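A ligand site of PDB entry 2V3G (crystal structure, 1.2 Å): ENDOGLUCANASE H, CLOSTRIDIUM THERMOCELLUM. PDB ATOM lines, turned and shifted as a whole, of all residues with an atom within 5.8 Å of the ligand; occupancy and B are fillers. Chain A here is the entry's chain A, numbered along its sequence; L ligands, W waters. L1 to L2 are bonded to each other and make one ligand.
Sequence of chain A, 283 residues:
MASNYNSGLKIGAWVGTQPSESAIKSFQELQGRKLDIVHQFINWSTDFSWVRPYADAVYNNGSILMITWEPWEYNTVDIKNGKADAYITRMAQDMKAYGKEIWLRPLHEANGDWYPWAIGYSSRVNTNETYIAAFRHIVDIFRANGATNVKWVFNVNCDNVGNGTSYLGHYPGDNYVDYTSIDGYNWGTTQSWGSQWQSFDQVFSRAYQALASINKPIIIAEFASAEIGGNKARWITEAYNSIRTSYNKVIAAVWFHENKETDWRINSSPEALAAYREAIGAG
NE1 of Trp 14 touches C5 of LIG L1, at 3.6 Å.
CB of Phe 41 touches O4 of LIG L1, 3.5 Å away.
Tyr 185 touches the ligand.
CH2 of Trp 187 touches O3 of LG2 L2 (3.6 Å).
Phe 256 touches the ligand.
Hydrophobic or aromatic side chains within 4 Å of the ligand: Trp 14, Phe 41, His 108, Tyr 115, Tyr 185, Trp 187 and Phe 256.
Of the 20 residues printed, 13 come within 4 Å of the ligand.
The side-chain carboxylate (OD1) of Asp 183 lies within hydrogen-bond range of the backbone NH (N) of Glu 222, at 3.3 Å.
NH2 of Arg 105 is in salt-bridge range of OE2 of Glu 222.
The side-chain hydroxyl (OH) of Tyr 115 lies within hydrogen-bond range of a ring nitrogen (NE2) of His 108, 3.1 Å away.
The side-chain carboxylate of Glu 258 sits at hydrogen-bond distance from the indole nitrogen of Trp 14, at 2.8 Å.
The backbone carbonyl oxygen (O) of Glu 258 sits close to the backbone NH (N) of Trp 264 (3.3 Å).
The side-chain carboxylate (OE1) of Glu 261 lies within hydrogen-bond range of the indole nitrogen (NE1) of Trp 264.
The side-chain carboxylate of Glu 109 sits close to the side-chain carboxylate of Asp 183 (2.4 Å).
The indole nitrogen of Trp 114 sits at hydrogen-bond distance from the side-chain carboxylate of Glu 109 (2.9 Å).
An oxygen (O2) of LIG L1 sits at hydrogen-bond distance from the side-chain carboxylate (OE2) of Glu 70, 2.6 Å away.
The side-chain carboxylate (OE1) of Glu 222 is in salt-bridge range of a nitrogen (N1) of LG2 L2.
The side-chain hydroxyl of Tyr 115 is in hydrogen-bond range of an oxygen (O2) of LIG L1, at 2.7 Å.
The side-chain carboxylate (OE1) of Glu 258 sits at hydrogen-bond distance from an oxygen (O6) of LIG L1 (2.7 Å).
OE2 of Glu 261 lies within hydrogen-bond range of O1 of LG2 L2 (2.8 Å).
N1 of LG2 L2 lies within salt-bridge range of OE2 of Glu 109 (2.8 Å).
The side-chain amino group (NZ) of Lys 260 sits at hydrogen-bond distance from an oxygen (O5) of LIG L1, 2.8 Å away.
A ring nitrogen (NE2) of His 108 lies within hydrogen-bond range of an oxygen (O2) of LG2 L2, 2.9 Å away.
Water W1 lies within hydrogen-bond range of O1 of LIG L1 (3.1 Å) and NZ of Lys 260 (3.4 Å).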
ATOM      1  N   TRP A  14     -11.842  24.477 -24.169  1.00  0.00           N
ATOM      2  CA  TRP A  14     -10.395  24.714 -24.007  1.00  0.00           C
ATOM      3  C   TRP A  14      -9.843  24.538 -25.407  1.00  0.00           C
ATOM      4  O   TRP A  14     -10.062  23.489 -26.035  1.00  0.00           O
ATOM      5  CB  TRP A  14      -9.805  23.660 -23.082  1.00  0.00           C
ATOM      6  CG  TRP A  14      -8.329  23.409 -23.211  1.00  0.00           C
ATOM      7  CD1 TRP A  14      -7.757  22.239 -23.615  1.00  0.00           C
ATOM      8  CD2 TRP A  14      -7.247  24.286 -22.859  1.00  0.00           C
ATOM      9  NE1 TRP A  14      -6.389  22.357 -23.570  1.00  0.00           N
ATOM     10  CE2 TRP A  14      -6.054  23.610 -23.130  1.00  0.00           C
ATOM     11  CE3 TRP A  14      -7.182  25.580 -22.353  1.00  0.00           C
ATOM     12  CZ2 TRP A  14      -4.802  24.193 -22.914  1.00  0.00           C
ATOM     13  CZ3 TRP A  14      -5.950  26.152 -22.147  1.00  0.00           C
ATOM     14  CH2 TRP A  14      -4.761  25.455 -22.416  1.00  0.00           C
ATOM     15  N   PHE A  41      -6.756  27.007 -18.045  1.00  0.00           N
ATOM     16  CA  PHE A  41      -6.191  26.356 -16.854  1.00  0.00           C
ATOM     17  C   PHE A  41      -5.090  27.226 -16.290  1.00  0.00           C
ATOM     18  O   PHE A  41      -4.210  27.667 -17.035  1.00  0.00           O
ATOM     19  CB  PHE A  41      -5.590  25.007 -17.211  1.00  0.00           C
ATOM     20  CG  PHE A  41      -6.582  23.978 -17.681  1.00  0.00           C
ATOM     21  CD1 PHE A  41      -7.094  23.028 -16.803  1.00  0.00           C
ATOM     22  CD2 PHE A  41      -7.021  23.922 -18.985  1.00  0.00           C
ATOM     23  CE1 PHE A  41      -8.015  22.073 -17.215  1.00  0.00           C
ATOM     24  CE2 PHE A  41      -7.913  22.984 -19.414  1.00  0.00           C
ATOM     25  CZ  PHE A  41      -8.419  22.071 -18.518  1.00  0.00           C
ATOM     26  N   THR A  68     -10.102  26.768 -14.741  1.00  0.00           N
ATOM     27  CA  THR A  68      -9.777  25.660 -13.869  1.00  0.00           C
ATOM     28  C   THR A  68      -8.517  26.038 -13.112  1.00  0.00           C
ATOM     29  O   THR A  68      -7.479  26.321 -13.699  1.00  0.00           O
ATOM     30  CB  THR A  68      -9.613  24.342 -14.659  1.00  0.00           C
ATOM     31  OG1 THR A  68     -10.859  24.009 -15.246  1.00  0.00           O
ATOM     32  CG2 THR A  68      -9.171  23.236 -13.768  1.00  0.00           C
ATOM     33  N   GLU A  70      -5.856  25.208 -10.525  1.00  0.00           N
ATOM     34  CA  GLU A  70      -5.192  23.971 -10.113  1.00  0.00           C
ATOM     35  C   GLU A  70      -4.143  24.200  -9.028  1.00  0.00           C
ATOM     36  O   GLU A  70      -3.090  24.755  -9.318  1.00  0.00           O
ATOM     37  CB  GLU A  70      -4.481  23.322 -11.310  1.00  0.00           C
ATOM     38  CG  GLU A  70      -5.403  22.940 -12.430  1.00  0.00           C
ATOM     39  CD  GLU A  70      -4.717  22.161 -13.527  1.00  0.00           C
ATOM     40  OE1 GLU A  70      -3.546  22.465 -13.855  1.00  0.00           O
ATOM     41  OE2 GLU A  70      -5.368  21.266 -14.059  1.00  0.00           O
ATOM     42  N   TRP A  72      -1.488  22.984  -7.642  1.00  0.00           N
ATOM     43  CA  TRP A  72      -0.267  22.179  -7.564  1.00  0.00           C
ATOM     44  C   TRP A  72       0.585  22.586  -6.371  1.00  0.00           C
ATOM     45  O   TRP A  72       1.303  21.786  -5.812  1.00  0.00           O
ATOM     46  CB  TRP A  72       0.534  22.294  -8.856  1.00  0.00           C
ATOM     47  CG  TRP A  72      -0.204  21.827 -10.076  1.00  0.00           C
ATOM     48  CD1 TRP A  72      -0.863  22.599 -10.966  1.00  0.00           C
ATOM     49  CD2 TRP A  72      -0.397  20.462 -10.497  1.00  0.00           C
ATOM     50  NE1 TRP A  72      -1.414  21.817 -11.944  1.00  0.00           N
ATOM     51  CE2 TRP A  72      -1.157  20.504 -11.679  1.00  0.00           C
ATOM     52  CE3 TRP A  72       0.030  19.226 -10.009  1.00  0.00           C
ATOM     53  CZ2 TRP A  72      -1.507  19.366 -12.382  1.00  0.00           C
ATOM     54  CZ3 TRP A  72      -0.333  18.094 -10.715  1.00  0.00           C
ATOM     55  CH2 TRP A  72      -1.082  18.175 -11.892  1.00  0.00           C
ATOM     56  N   ARG A 105     -13.374  26.964 -11.274  1.00  0.00           N
ATOM     57  CA  ARG A 105     -13.418  25.528 -11.022  1.00  0.00           C
ATOM     58  C   ARG A 105     -12.139  25.122 -10.297  1.00  0.00           C
ATOM     59  O   ARG A 105     -11.178  24.658 -10.910  1.00  0.00           O
ATOM     60  CB  ARG A 105     -13.593  24.791 -12.354  1.00  0.00           C
ATOM     61  CG  ARG A 105     -13.906  23.340 -12.193  1.00  0.00           C
ATOM     62  CD  ARG A 105     -14.157  22.652 -13.511  1.00  0.00           C
ATOM     63  NE  ARG A 105     -12.967  22.465 -14.326  1.00  0.00           N
ATOM     64  CZ  ARG A 105     -12.593  21.336 -14.961  1.00  0.00           C
ATOM     65  NH1 ARG A 105     -13.226  20.213 -14.809  1.00  0.00           N
ATOM     66  NH2 ARG A 105     -11.500  21.353 -15.726  1.00  0.00           N
ATOM     67  N   HIS A 108     -10.379  20.467  -9.126  1.00  0.00           N
ATOM     68  CA  HIS A 108     -11.208  19.619  -9.958  1.00  0.00           C
ATOM     69  C   HIS A 108     -10.774  18.154  -9.940  1.00  0.00           C
ATOM     70  O   HIS A 108      -9.667  17.791  -9.481  1.00  0.00           O
ATOM     71  CB  HIS A 108     -11.271  20.173 -11.383  1.00  0.00           C
ATOM     72  CG  HIS A 108     -10.099  19.890 -12.256  1.00  0.00           C
ATOM     73  ND1 HIS A 108      -8.839  20.397 -12.000  1.00  0.00           N
ATOM     74  CD2 HIS A 108     -10.026  19.209 -13.427  1.00  0.00           C
ATOM     75  CE1 HIS A 108      -8.038  19.978 -12.960  1.00  0.00           C
ATOM     76  NE2 HIS A 108      -8.731  19.278 -13.847  1.00  0.00           N
ATOM     77  N   GLU A 109     -11.648  17.294 -10.445  1.00  0.00           N
ATOM     78  CA  GLU A 109     -11.395  15.851 -10.564  1.00  0.00           C
ATOM     79  C   GLU A 109     -10.850  15.261  -9.267  1.00  0.00           C
ATOM     80  O   GLU A 109      -9.967  14.393  -9.262  1.00  0.00           O
ATOM     81  CB  GLU A 109     -10.495  15.514 -11.761  1.00  0.00           C
ATOM     82  CG  GLU A 109     -11.182  15.762 -13.086  1.00  0.00           C
ATOM     83  CD  GLU A 109     -10.277  15.636 -14.303  1.00  0.00           C
ATOM     84  OE1 GLU A 109      -9.149  15.197 -14.184  1.00  0.00           O
ATOM     85  OE2 GLU A 109     -10.726  15.965 -15.433  1.00  0.00           O
ATOM     86  N   TRP A 114      -4.984  11.376  -9.607  1.00  0.00           N
ATOM     87  CA  TRP A 114      -3.848  11.952 -10.323  1.00  0.00           C
ATOM     88  C   TRP A 114      -3.456  13.333  -9.889  1.00  0.00           C
ATOM     89  O   TRP A 114      -2.341  13.743 -10.166  1.00  0.00           O
ATOM     90  CB  TRP A 114      -4.046  11.894 -11.857  1.00  0.00           C
ATOM     91  CG  TRP A 114      -5.412  12.351 -12.287  1.00  0.00           C
ATOM     92  CD1 TRP A 114      -5.829  13.597 -12.562  1.00  0.00           C
ATOM     93  CD2 TRP A 114      -6.543  11.505 -12.511  1.00  0.00           C
ATOM     94  NE1 TRP A 114      -7.151  13.611 -12.892  1.00  0.00           N
ATOM     95  CE2 TRP A 114      -7.611  12.330 -12.875  1.00  0.00           C
ATOM     96  CE3 TRP A 114      -6.760  10.124 -12.431  1.00  0.00           C
ATOM     97  CZ2 TRP A 114      -8.875  11.802 -13.191  1.00  0.00           C
ATOM     98  CZ3 TRP A 114      -8.011   9.617 -12.729  1.00  0.00           C
ATOM     99  CH2 TRP A 114      -9.042  10.451 -13.094  1.00  0.00           C
ATOM    100  N   TYR A 115      -4.293  14.049  -9.167  1.00  0.00           N
ATOM    101  CA  TYR A 115      -3.929  15.386  -8.706  1.00  0.00           C
ATOM    102  C   TYR A 115      -3.590  15.347  -7.221  1.00  0.00           C
ATOM    103  O   TYR A 115      -4.183  14.606  -6.447  1.00  0.00           O
ATOM    104  CB  TYR A 115      -5.072  16.360  -8.925  1.00  0.00           C
ATOM    105  CG  TYR A 115      -5.351  16.627 -10.384  1.00  0.00           C
ATOM    106  CD1 TYR A 115      -4.331  16.998 -11.250  1.00  0.00           C
ATOM    107  CD2 TYR A 115      -6.622  16.626 -10.883  1.00  0.00           C
ATOM    108  CE1 TYR A 115      -4.573  17.291 -12.574  1.00  0.00           C
ATOM    109  CE2 TYR A 115      -6.872  16.902 -12.215  1.00  0.00           C
ATOM    110  CZ  TYR A 115      -5.873  17.247 -13.047  1.00  0.00           C
ATOM    111  OH  TYR A 115      -6.160  17.534 -14.366  1.00  0.00           O
ATOM    112  N   ASN A 157     -14.766  13.725 -11.973  1.00  0.00           N
ATOM    113  CA  ASN A 157     -14.435  12.858 -13.086  1.00  0.00           C
ATOM    114  C   ASN A 157     -15.577  11.878 -13.306  1.00  0.00           C
ATOM    115  O   ASN A 157     -16.285  11.501 -12.370  1.00  0.00           O
ATOM    116  CB  ASN A 157     -13.178  12.078 -12.775  1.00  0.00           C
ATOM    117  CG  ASN A 157     -12.612  11.384 -13.965  1.00  0.00           C
ATOM    118  OD1 ASN A 157     -12.462  10.114 -13.974  1.00  0.00           O
ATOM    119  ND2 ASN A 157     -12.328  12.128 -14.962  1.00  0.00           N
ATOM    120  N   ASP A 183     -16.231  15.767 -16.042  1.00  0.00           N
ATOM    121  CA  ASP A 183     -15.243  15.600 -17.085  1.00  0.00           C
ATOM    122  C   ASP A 183     -15.259  14.152 -17.539  1.00  0.00           C
ATOM    123  O   ASP A 183     -15.389  13.227 -16.719  1.00  0.00           O
ATOM    124  CB  ASP A 183     -13.840  15.878 -16.554  1.00  0.00           C
ATOM    125  CG  ASP A 183     -13.623  17.312 -16.193  1.00  0.00           C
ATOM    126  OD1 ASP A 183     -14.533  18.146 -16.353  1.00  0.00           O
ATOM    127  OD2 ASP A 183     -12.499  17.635 -15.689  1.00  0.00           O
ATOM    128  N   TYR A 185     -13.983  11.329 -21.079  1.00  0.00           N
ATOM    129  CA  TYR A 185     -13.382  11.139 -22.373  1.00  0.00           C
ATOM    130  C   TYR A 185     -13.686   9.751 -22.916  1.00  0.00           C
ATOM    131  O   TYR A 185     -13.675   8.762 -22.175  1.00  0.00           O
ATOM    132  CB  TYR A 185     -11.839  11.285 -22.258  1.00  0.00           C
ATOM    133  CG  TYR A 185     -11.424  12.688 -21.972  1.00  0.00           C
ATOM    134  CD1 TYR A 185     -10.998  13.510 -22.994  1.00  0.00           C
ATOM    135  CD2 TYR A 185     -11.505  13.229 -20.690  1.00  0.00           C
ATOM    136  CE1 TYR A 185     -10.639  14.833 -22.737  1.00  0.00           C
ATOM    137  CE2 TYR A 185     -11.192  14.581 -20.459  1.00  0.00           C
ATOM    138  CZ  TYR A 185     -10.751  15.350 -21.480  1.00  0.00           C
ATOM    139  OH  TYR A 185     -10.385  16.659 -21.286  1.00  0.00           O
ATOM    140  N   TRP A 187     -11.743   7.318 -24.734  1.00  0.00           N
ATOM    141  CA  TRP A 187     -10.343   7.032 -25.021  1.00  0.00           C
ATOM    142  C   TRP A 187     -10.165   6.131 -26.241  1.00  0.00           C
ATOM    143  O   TRP A 187      -9.061   5.943 -26.742  1.00  0.00           O
ATOM    144  CB  TRP A 187      -9.697   6.361 -23.805  1.00  0.00           C
ATOM    145  CG  TRP A 187      -9.614   7.241 -22.634  1.00  0.00           C
ATOM    146  CD1 TRP A 187     -10.558   7.429 -21.663  1.00  0.00           C
ATOM    147  CD2 TRP A 187      -8.535   8.095 -22.281  1.00  0.00           C
ATOM    148  NE1 TRP A 187     -10.152   8.355 -20.758  1.00  0.00           N
ATOM    149  CE2 TRP A 187      -8.898   8.754 -21.096  1.00  0.00           C
ATOM    150  CE3 TRP A 187      -7.293   8.363 -22.837  1.00  0.00           C
ATOM    151  CZ2 TRP A 187      -8.069   9.678 -20.470  1.00  0.00           C
ATOM    152  CZ3 TRP A 187      -6.472   9.236 -22.187  1.00  0.00           C
ATOM    153  CH2 TRP A 187      -6.870   9.888 -21.039  1.00  0.00           C
ATOM    154  N   GLU A 222     -15.279  19.222 -19.384  1.00  0.00           N
ATOM    155  CA  GLU A 222     -14.327  18.691 -20.331  1.00  0.00           C
ATOM    156  C   GLU A 222     -14.915  17.453 -20.964  1.00  0.00           C
ATOM    157  O   GLU A 222     -15.339  16.543 -20.230  1.00  0.00           O
ATOM    158  CB  GLU A 222     -13.001  18.267 -19.701  1.00  0.00           C
ATOM    159  CG  GLU A 222     -12.215  19.318 -18.970  1.00  0.00           C
ATOM    160  CD  GLU A 222     -10.915  18.780 -18.405  1.00  0.00           C
ATOM    161  OE1 GLU A 222     -10.475  17.686 -18.839  1.00  0.00           O
ATOM    162  OE2 GLU A 222     -10.317  19.444 -17.529  1.00  0.00           O
ATOM    163  N   PHE A 256     -12.663  19.659 -24.968  1.00  0.00           N
ATOM    164  CA  PHE A 256     -11.242  19.737 -24.659  1.00  0.00           C
ATOM    165  C   PHE A 256     -10.476  19.544 -25.972  1.00  0.00           C
ATOM    166  O   PHE A 256     -10.268  18.429 -26.432  1.00  0.00           O
ATOM    167  CB  PHE A 256     -10.864  18.658 -23.647  1.00  0.00           C
ATOM    168  CG  PHE A 256      -9.468  18.765 -23.110  1.00  0.00           C
ATOM    169  CD1 PHE A 256      -9.210  19.507 -21.977  1.00  0.00           C
ATOM    170  CD2 PHE A 256      -8.443  18.049 -23.673  1.00  0.00           C
ATOM    171  CE1 PHE A 256      -7.937  19.529 -21.442  1.00  0.00           C
ATOM    172  CE2 PHE A 256      -7.174  18.075 -23.146  1.00  0.00           C
ATOM    173  CZ  PHE A 256      -6.927  18.805 -22.027  1.00  0.00           C
ATOM    174  N   GLU A 258      -7.320  19.548 -27.785  1.00  0.00           N
ATOM    175  CA  GLU A 258      -5.864  19.490 -27.671  1.00  0.00           C
ATOM    176  C   GLU A 258      -5.398  18.138 -28.177  1.00  0.00           C
ATOM    177  O   GLU A 258      -6.037  17.116 -27.889  1.00  0.00           O
ATOM    178  CB  GLU A 258      -5.398  19.720 -26.218  1.00  0.00           C
ATOM    179  CG  GLU A 258      -3.896  19.990 -26.113  1.00  0.00           C
ATOM    180  CD  GLU A 258      -3.416  20.202 -24.690  1.00  0.00           C
ATOM    181  OE1 GLU A 258      -4.188  20.606 -23.815  1.00  0.00           O
ATOM    182  OE2 GLU A 258      -2.216  19.951 -24.449  1.00  0.00           O
ATOM    183  N   LYS A 260      -3.145  15.629 -27.270  1.00  0.00           N
ATOM    184  CA  LYS A 260      -2.487  15.419 -25.985  1.00  0.00           C
ATOM    185  C   LYS A 260      -2.315  13.931 -25.767  1.00  0.00           C
ATOM    186  O   LYS A 260      -1.534  13.309 -26.496  1.00  0.00           O
ATOM    187  CB  LYS A 260      -3.222  16.183 -24.886  1.00  0.00           C
ATOM    188  CG  LYS A 260      -2.446  16.302 -23.571  1.00  0.00           C
ATOM    189  CD  LYS A 260      -3.203  17.060 -22.527  1.00  0.00           C
ATOM    190  CE  LYS A 260      -2.396  17.145 -21.246  1.00  0.00           C
ATOM    191  NZ  LYS A 260      -3.137  17.919 -20.200  1.00  0.00           N
ATOM    192  N   GLU A 261      -3.049  13.312 -24.856  1.00  0.00           N
ATOM    193  CA  GLU A 261      -2.931  11.892 -24.611  1.00  0.00           C
ATOM    194  C   GLU A 261      -3.320  11.107 -25.854  1.00  0.00           C
ATOM    195  O   GLU A 261      -2.759  10.042 -26.131  1.00  0.00           O
ATOM    196  CB  GLU A 261      -3.774  11.486 -23.414  1.00  0.00           C
ATOM    197  CG  GLU A 261      -3.418  12.216 -22.110  1.00  0.00           C
ATOM    198  CD  GLU A 261      -4.183  13.510 -21.855  1.00  0.00           C
ATOM    199  OE1 GLU A 261      -4.807  14.056 -22.790  1.00  0.00           O
ATOM    200  OE2 GLU A 261      -4.186  13.959 -20.688  1.00  0.00           O
ATOM    201  N   TRP A 264      -7.598  14.631 -29.288  1.00  0.00           N
ATOM    202  CA  TRP A 264      -8.928  15.016 -28.854  1.00  0.00           C
ATOM    203  C   TRP A 264      -9.553  16.082 -29.742  1.00  0.00           C
ATOM    204  O   TRP A 264     -10.726  16.357 -29.646  1.00  0.00           O
ATOM    205  CB  TRP A 264      -8.862  15.594 -27.435  1.00  0.00           C
ATOM    206  CG  TRP A 264      -8.289  14.709 -26.393  1.00  0.00           C
ATOM    207  CD1 TRP A 264      -7.233  15.040 -25.590  1.00  0.00           C
ATOM    208  CD2 TRP A 264      -8.728  13.427 -25.963  1.00  0.00           C
ATOM    209  NE1 TRP A 264      -6.983  14.035 -24.698  1.00  0.00           N
ATOM    210  CE2 TRP A 264      -7.888  13.033 -24.908  1.00  0.00           C
ATOM    211  CE3 TRP A 264      -9.728  12.541 -26.411  1.00  0.00           C
ATOM    212  CZ2 TRP A 264      -8.053  11.835 -24.238  1.00  0.00           C
ATOM    213  CZ3 TRP A 264      -9.885  11.334 -25.725  1.00  0.00           C
ATOM    214  CH2 TRP A 264      -9.042  10.994 -24.665  1.00  0.00           C
HETATM  215  C1  LIG L   1      -4.116  19.593 -16.759  1.00  0.00           C
HETATM  216  C2  LIG L   1      -3.732  21.064 -16.867  1.00  0.00           C
HETATM  217  C3  LIG L   1      -3.494  21.394 -18.327  1.00  0.00           C
HETATM  218  C4  LIG L   1      -4.750  21.039 -19.123  1.00  0.00           C
HETATM  219  C5  LIG L   1      -4.637  21.363 -20.613  1.00  0.00           C
HETATM  220  C6  LIG L   1      -5.280  19.266 -17.669  1.00  0.00           C
HETATM  221  O1  LIG L   1      -5.432  17.852 -17.665  1.00  0.00           O
HETATM  222  O2  LIG L   1      -4.405  19.255 -15.403  1.00  0.00           O
HETATM  223  O3  LIG L   1      -2.593  21.359 -16.088  1.00  0.00           O
HETATM  224  O4  LIG L   1      -3.234  22.780 -18.438  1.00  0.00           O
HETATM  225  O5  LIG L   1      -4.990  19.638 -18.993  1.00  0.00           O
HETATM  226  O6  LIG L   1      -3.587  20.548 -21.182  1.00  0.00           O
HETATM  227  O1  LG2 L   2      -5.470  16.307 -20.020  1.00  0.00           O
HETATM  228  C1  LG2 L   2      -6.299  16.018 -18.876  1.00  0.00           C
HETATM  229  C2  LG2 L   2      -6.645  17.350 -18.202  1.00  0.00           C
HETATM  230  C3  LG2 L   2      -7.610  17.121 -17.009  1.00  0.00           C
HETATM  231  N1  LG2 L   2      -8.774  16.318 -17.405  1.00  0.00           N
HETATM  232  C4  LG2 L   2      -8.431  15.037 -18.061  1.00  0.00           C
HETATM  233  C5  LG2 L   2      -7.593  15.327 -19.308  1.00  0.00           C
HETATM  234  C6  LG2 L   2      -7.364  14.014 -20.090  1.00  0.00           C
HETATM  235  O2  LG2 L   2      -8.107  18.347 -16.496  1.00  0.00           O
HETATM  236  O3  LG2 L   2      -6.642  13.054 -19.350  1.00  0.00           O
HETATM  237  O   HOH W   1      -2.861  16.075 -17.355  1.00  0.00           O
HETATM  238  O   HOH W   2      -1.633  23.271 -20.611  1.00  0.00           O
HETATM  239  O   HOH W   3      -8.258  11.668 -17.429  1.00  0.00           O
